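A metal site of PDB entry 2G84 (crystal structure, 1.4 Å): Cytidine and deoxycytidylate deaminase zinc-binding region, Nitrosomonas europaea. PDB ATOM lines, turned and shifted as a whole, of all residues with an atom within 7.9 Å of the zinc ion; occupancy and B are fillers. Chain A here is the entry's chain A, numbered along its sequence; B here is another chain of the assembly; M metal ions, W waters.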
ATOM      1  N   PHE A  50      24.662   9.576 -14.273  1.00  0.00           N
ATOM      2  CA  PHE A  50      23.580  10.448 -14.746  1.00  0.00           C
ATOM      3  C   PHE A  50      23.117   9.997 -16.095  1.00  0.00           C
ATOM      4  O   PHE A  50      23.926   9.685 -16.987  1.00  0.00           O
ATOM      5  CB  PHE A  50      24.021  11.913 -14.818  1.00  0.00           C
ATOM      6  CG  PHE A  50      24.504  12.452 -13.499  1.00  0.00           C
ATOM      7  CD1 PHE A  50      23.597  12.834 -12.514  1.00  0.00           C
ATOM      8  CD2 PHE A  50      25.894  12.519 -13.222  1.00  0.00           C
ATOM      9  CE1 PHE A  50      24.047  13.283 -11.276  1.00  0.00           C
ATOM     10  CE2 PHE A  50      26.333  12.969 -11.971  1.00  0.00           C
ATOM     11  CZ  PHE A  50      25.418  13.334 -10.997  1.00  0.00           C
ATOM     12  N   ASN A  68      25.860  10.899 -19.034  1.00  0.00           N
ATOM     13  CA  ASN A  68      27.068  11.695 -18.823  1.00  0.00           C
ATOM     14  C   ASN A  68      28.276  10.987 -19.444  1.00  0.00           C
ATOM     15  O   ASN A  68      28.632   9.878 -19.009  1.00  0.00           O
ATOM     16  CB  ASN A  68      27.234  11.897 -17.305  1.00  0.00           C
ATOM     17  CG  ASN A  68      28.423  12.741 -16.939  1.00  0.00           C
ATOM     18  OD1 ASN A  68      28.324  13.696 -16.167  1.00  0.00           O
ATOM     19  ND2 ASN A  68      29.564  12.376 -17.424  1.00  0.00           N
ATOM     20  N   VAL A  70      31.213  12.937 -19.893  1.00  0.00           N
ATOM     21  CA  VAL A  70      32.180  14.040 -19.725  1.00  0.00           C
ATOM     22  C   VAL A  70      33.630  13.568 -19.686  1.00  0.00           C
ATOM     23  O   VAL A  70      34.484  14.041 -20.478  1.00  0.00           O
ATOM     24  CB  VAL A  70      31.882  14.824 -18.421  1.00  0.00           C
ATOM     25  CG1 VAL A  70      33.050  15.788 -18.067  1.00  0.00           C
ATOM     26  CG2 VAL A  70      30.576  15.595 -18.567  1.00  0.00           C
ATOM     27  N   SER A  76      33.395  18.586 -21.468  1.00  0.00           N
ATOM     28  CA  SER A  76      32.719  19.003 -20.248  1.00  0.00           C
ATOM     29  C   SER A  76      31.246  19.292 -20.497  1.00  0.00           C
ATOM     30  O   SER A  76      30.458  19.276 -19.538  1.00  0.00           O
ATOM     31  CB  SER A  76      33.429  20.185 -19.584  1.00  0.00           C
ATOM     32  OG  SER A  76      33.443  21.311 -20.445  1.00  0.00           O
ATOM     33  N   ALA A  77      30.856  19.541 -21.754  1.00  0.00           N
ATOM     34  CA  ALA A  77      29.425  19.804 -22.071  1.00  0.00           C
ATOM     35  C   ALA A  77      28.602  18.540 -22.203  1.00  0.00           C
ATOM     36  O   ALA A  77      27.385  18.643 -22.374  1.00  0.00           O
ATOM     37  CB  ALA A  77      29.291  20.630 -23.348  1.00  0.00           C
ATOM     38  N   ALA A  78      29.255  17.362 -22.162  1.00  0.00           N
ATOM     39  CA  ALA A  78      28.561  16.090 -22.465  1.00  0.00           C
ATOM     40  C   ALA A  78      27.800  15.552 -21.242  1.00  0.00           C
ATOM     41  O   ALA A  78      27.923  14.374 -20.824  1.00  0.00           O
ATOM     42  CB  ALA A  78      29.536  15.039 -23.048  1.00  0.00           C
ATOM     43  N   HIS A  79      26.995  16.427 -20.645  1.00  0.00           N
ATOM     44  CA  HIS A  79      26.051  15.993 -19.628  1.00  0.00           C
ATOM     45  C   HIS A  79      24.913  15.235 -20.254  1.00  0.00           C
ATOM     46  O   HIS A  79      24.582  15.423 -21.424  1.00  0.00           O
ATOM     47  CB  HIS A  79      25.502  17.213 -18.878  1.00  0.00           C
ATOM     48  CG  HIS A  79      26.500  17.859 -17.978  1.00  0.00           C
ATOM     49  ND1 HIS A  79      26.154  18.688 -16.932  1.00  0.00           N
ATOM     50  CD2 HIS A  79      27.858  17.774 -17.949  1.00  0.00           C
ATOM     51  CE1 HIS A  79      27.241  19.111 -16.321  1.00  0.00           C
ATOM     52  NE2 HIS A  79      28.291  18.561 -16.915  1.00  0.00           N
ATOM     53  N   ALA A  80      24.291  14.393 -19.441  1.00  0.00           N
ATOM     54  CA  ALA A  80      23.189  13.546 -19.923  1.00  0.00           C
ATOM     55  C   ALA A  80      22.071  14.349 -20.641  1.00  0.00           C
ATOM     56  O   ALA A  80      21.583  13.955 -21.710  1.00  0.00           O
ATOM     57  CB  ALA A  80      22.552  12.828 -18.706  1.00  0.00           C
ATOM     58  N   GLU A  81      21.732  15.499 -20.038  1.00  0.00           N
ATOM     59  CA  GLU A  81      20.627  16.302 -20.573  1.00  0.00           C
ATOM     60  C   GLU A  81      20.997  16.886 -21.948  1.00  0.00           C
ATOM     61  O   GLU A  81      20.173  16.942 -22.855  1.00  0.00           O
ATOM     62  CB  GLU A  81      20.318  17.460 -19.608  1.00  0.00           C
ATOM     63  CG  GLU A  81      19.937  17.015 -18.188  1.00  0.00           C
ATOM     64  CD  GLU A  81      21.117  17.002 -17.214  1.00  0.00           C
ATOM     65  OE1 GLU A  81      22.133  16.375 -17.523  1.00  0.00           O
ATOM     66  OE2 GLU A  81      21.027  17.648 -16.125  1.00  0.00           O
ATOM     67  N   ILE A  82      22.230  17.348 -22.100  1.00  0.00           N
ATOM     68  CA  ILE A  82      22.676  17.926 -23.353  1.00  0.00           C
ATOM     69  C   ILE A  82      22.637  16.875 -24.445  1.00  0.00           C
ATOM     70  O   ILE A  82      22.186  17.112 -25.551  1.00  0.00           O
ATOM     71  CB  ILE A  82      24.127  18.514 -23.223  1.00  0.00           C
ATOM     72  CG1 ILE A  82      24.222  19.587 -22.135  1.00  0.00           C
ATOM     73  CG2 ILE A  82      24.623  19.012 -24.598  1.00  0.00           C
ATOM     74  CD1 ILE A  82      23.338  20.750 -22.363  1.00  0.00           C
ATOM     75  N   ALA A 111      18.609  13.287 -12.297  1.00  0.00           N
ATOM     76  CA  ALA A 111      18.904  14.247 -11.238  1.00  0.00           C
ATOM     77  C   ALA A 111      18.524  15.653 -11.710  1.00  0.00           C
ATOM     78  O   ALA A 111      18.490  15.924 -12.912  1.00  0.00           O
ATOM     79  CB  ALA A 111      20.387  14.207 -10.880  1.00  0.00           C
ATOM     80  N   GLU A 112      18.305  16.561 -10.764  1.00  0.00           N
ATOM     81  CA  GLU A 112      18.007  17.951 -11.145  1.00  0.00           C
ATOM     82  C   GLU A 112      19.186  18.520 -11.948  1.00  0.00           C
ATOM     83  O   GLU A 112      20.352  18.217 -11.667  1.00  0.00           O
ATOM     84  CB  GLU A 112      17.732  18.785  -9.886  1.00  0.00           C
ATOM     85  CG  GLU A 112      16.377  18.382  -9.230  1.00  0.00           C
ATOM     86  CD  GLU A 112      16.090  19.053  -7.914  1.00  0.00           C
ATOM     87  OE1 GLU A 112      16.921  19.843  -7.422  1.00  0.00           O
ATOM     88  OE2 GLU A 112      15.012  18.718  -7.347  1.00  0.00           O
ATOM     89  N   PRO A 113      18.876  19.392 -12.934  1.00  0.00           N
ATOM     90  CA  PRO A 113      19.921  19.892 -13.839  1.00  0.00           C
ATOM     91  C   PRO A 113      20.853  20.914 -13.219  1.00  0.00           C
ATOM     92  O   PRO A 113      20.428  21.721 -12.396  1.00  0.00           O
ATOM     93  CB  PRO A 113      19.127  20.592 -14.963  1.00  0.00           C
ATOM     94  CG  PRO A 113      17.856  21.029 -14.271  1.00  0.00           C
ATOM     95  CD  PRO A 113      17.530  19.877 -13.324  1.00  0.00           C
ATOM     96  N   CYS A 114      22.119  20.875 -13.669  1.00  0.00           N
ATOM     97  CA  CYS A 114      23.059  21.918 -13.320  1.00  0.00           C
ATOM     98  C   CYS A 114      22.671  23.199 -14.062  1.00  0.00           C
ATOM     99  O   CYS A 114      21.776  23.200 -14.908  1.00  0.00           O
ATOM    100  CB  CYS A 114      24.494  21.516 -13.689  1.00  0.00           C
ATOM    101  SG  CYS A 114      24.856  21.608 -15.475  1.00  0.00           S
ATOM    102  N   VAL A 115      23.399  24.286 -13.797  1.00  0.00           N
ATOM    103  CA  VAL A 115      23.056  25.565 -14.432  1.00  0.00           C
ATOM    104  C   VAL A 115      23.185  25.514 -15.960  1.00  0.00           C
ATOM    105  O   VAL A 115      22.354  26.106 -16.653  1.00  0.00           O
ATOM    106  CB  VAL A 115      23.817  26.738 -13.824  1.00  0.00           C
ATOM    107  CG1 VAL A 115      25.353  26.563 -13.900  1.00  0.00           C
ATOM    108  CG2 VAL A 115      23.327  28.058 -14.444  1.00  0.00           C
ATOM    109  N   MET A 116      24.205  24.830 -16.485  1.00  0.00           N
ATOM    110  CA  MET A 116      24.315  24.670 -17.937  1.00  0.00           C
ATOM    111  C   MET A 116      23.070  23.964 -18.503  1.00  0.00           C
ATOM    112  O   MET A 116      22.495  24.425 -19.498  1.00  0.00           O
ATOM    113  CB  MET A 116      25.560  23.829 -18.285  1.00  0.00           C
ATOM    114  CG  MET A 116      25.706  23.559 -19.780  1.00  0.00           C
ATOM    115  SD  MET A 116      27.231  22.631 -20.134  1.00  0.00           S
ATOM    116  CE  MET A 116      26.835  21.040 -19.409  1.00  0.00           C
ATOM    117  N   CYS A 117      22.697  22.837 -17.919  1.00  0.00           N
ATOM    118  CA  CYS A 117      21.589  22.048 -18.454  1.00  0.00           C
ATOM    119  C   CYS A 117      20.246  22.736 -18.230  1.00  0.00           C
ATOM    120  O   CYS A 117      19.310  22.559 -19.003  1.00  0.00           O
ATOM    121  CB  CYS A 117      21.622  20.679 -17.825  1.00  0.00           C
ATOM    122  SG  CYS A 117      23.077  19.750 -18.464  1.00  0.00           S
ATOM    123  N   PHE A 118      20.143  23.492 -17.138  1.00  0.00           N
ATOM    124  CA  PHE A 118      18.980  24.346 -16.925  1.00  0.00           C
ATOM    125  C   PHE A 118      18.787  25.277 -18.126  1.00  0.00           C
ATOM    126  O   PHE A 118      17.668  25.384 -18.665  1.00  0.00           O
ATOM    127  CB  PHE A 118      19.186  25.139 -15.598  1.00  0.00           C
ATOM    128  CG  PHE A 118      18.291  26.340 -15.411  1.00  0.00           C
ATOM    129  CD1 PHE A 118      16.951  26.204 -15.079  1.00  0.00           C
ATOM    130  CD2 PHE A 118      18.829  27.616 -15.500  1.00  0.00           C
ATOM    131  CE1 PHE A 118      16.146  27.339 -14.869  1.00  0.00           C
ATOM    132  CE2 PHE A 118      18.055  28.770 -15.297  1.00  0.00           C
ATOM    133  CZ  PHE A 118      16.683  28.614 -14.981  1.00  0.00           C
ATOM    134  N   ALA A 120      20.018  24.798 -21.146  1.00  0.00           N
ATOM    135  CA  ALA A 120      19.737  23.985 -22.325  1.00  0.00           C
ATOM    136  C   ALA A 120      18.264  23.558 -22.349  1.00  0.00           C
ATOM    137  O   ALA A 120      17.668  23.493 -23.428  1.00  0.00           O
ATOM    138  CB  ALA A 120      20.626  22.767 -22.291  1.00  0.00           C
ATOM    139  N   ASP A 144      28.711  19.209  -8.399  1.00  0.00           N
ATOM    140  CA  ASP A 144      28.313  20.589  -8.209  1.00  0.00           C
ATOM    141  C   ASP A 144      27.226  20.907  -9.222  1.00  0.00           C
ATOM    142  O   ASP A 144      27.395  20.589 -10.405  1.00  0.00           O
ATOM    143  CB  ASP A 144      29.548  21.425  -8.518  1.00  0.00           C
ATOM    144  CG  ASP A 144      29.432  22.879  -8.094  1.00  0.00           C
ATOM    145  OD1 ASP A 144      28.345  23.380  -7.697  1.00  0.00           O
ATOM    146  OD2 ASP A 144      30.523  23.529  -8.145  1.00  0.00           O
ATOM    147  N   GLU A 145      26.120  21.507  -8.768  1.00  0.00           N
ATOM    148  CA  GLU A 145      25.084  22.000  -9.714  1.00  0.00           C
ATOM    149  C   GLU A 145      25.406  23.388 -10.274  1.00  0.00           C
ATOM    150  O   GLU A 145      24.792  23.838 -11.276  1.00  0.00           O
ATOM    151  CB  GLU A 145      23.707  22.057  -9.045  1.00  0.00           C
ATOM    152  CG  GLU A 145      23.162  20.714  -8.578  1.00  0.00           C
ATOM    153  CD  GLU A 145      22.587  19.843  -9.704  1.00  0.00           C
ATOM    154  OE1 GLU A 145      23.132  19.864 -10.810  1.00  0.00           O
ATOM    155  OE2 GLU A 145      21.597  19.122  -9.454  1.00  0.00           O
ATOM    156  N   TRP B 123      32.199  24.775 -16.210  1.00  0.00           N
ATOM    157  CA  TRP B 123      32.646  23.401 -16.182  1.00  0.00           C
ATOM    158  C   TRP B 123      33.867  23.162 -17.061  1.00  0.00           C
ATOM    159  O   TRP B 123      34.517  22.115 -16.961  1.00  0.00           O
ATOM    160  CB  TRP B 123      31.548  22.423 -16.606  1.00  0.00           C
ATOM    161  CG  TRP B 123      30.276  22.558 -15.843  1.00  0.00           C
ATOM    162  CD1 TRP B 123      29.018  22.538 -16.381  1.00  0.00           C
ATOM    163  CD2 TRP B 123      30.098  22.761 -14.432  1.00  0.00           C
ATOM    164  NE1 TRP B 123      28.074  22.704 -15.396  1.00  0.00           N
ATOM    165  CE2 TRP B 123      28.701  22.855 -14.186  1.00  0.00           C
ATOM    166  CE3 TRP B 123      30.991  22.844 -13.327  1.00  0.00           C
ATOM    167  CZ2 TRP B 123      28.173  23.027 -12.897  1.00  0.00           C
ATOM    168  CZ3 TRP B 123      30.449  23.032 -12.043  1.00  0.00           C
ATOM    169  CH2 TRP B 123      29.054  23.130 -11.847  1.00  0.00           C
HETATM  170 ZN    ZN M   1      24.337  19.612 -16.578  1.00  0.00          ZN
HETATM  171  O   HOH W   1      23.235  18.569 -15.152  1.00  0.00           O
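NE1 of Trp 123 of chain B lies close to SG of Cys 114, 3.4 Å away. NE2 of His 79 lies close to O of Ser 76 (3.5 Å). The side-chain sulfur (SG) of Cys 114 sits close to the backbone NH (N) of Met 116, at 3.4 Å. The side-chain carboxylate of Glu 81 lies close to the side-chain sulfur of Cys 117. The backbone NH (N) of Cys 114 sits at hydrogen-bond distance from the side-chain carboxylate (OE1) of Glu 145 (3.2 Å).
Water W1 bridges OE2 of Glu 81 (2.6 Å) and N of Cys 114 (3.0 Å).
The zinc ion is bound by ND1 of His 79 (2.1 Å), water W1 (2.1 Å), SG of Cys 117 (2.3 Å) and SG of Cys 114 (2.3 Å). The zinc ion has four donor atoms within binding distance.
Residues that only touch the zinc ion: Glu 81 (3.9 Å). Four residues have an atom within 4 Å of the zinc ion: His 79, Glu 81, Cys 114 and Cys 117. The nearest printed residue that does not touch the zinc ion is Met 116 (4.04 Å).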
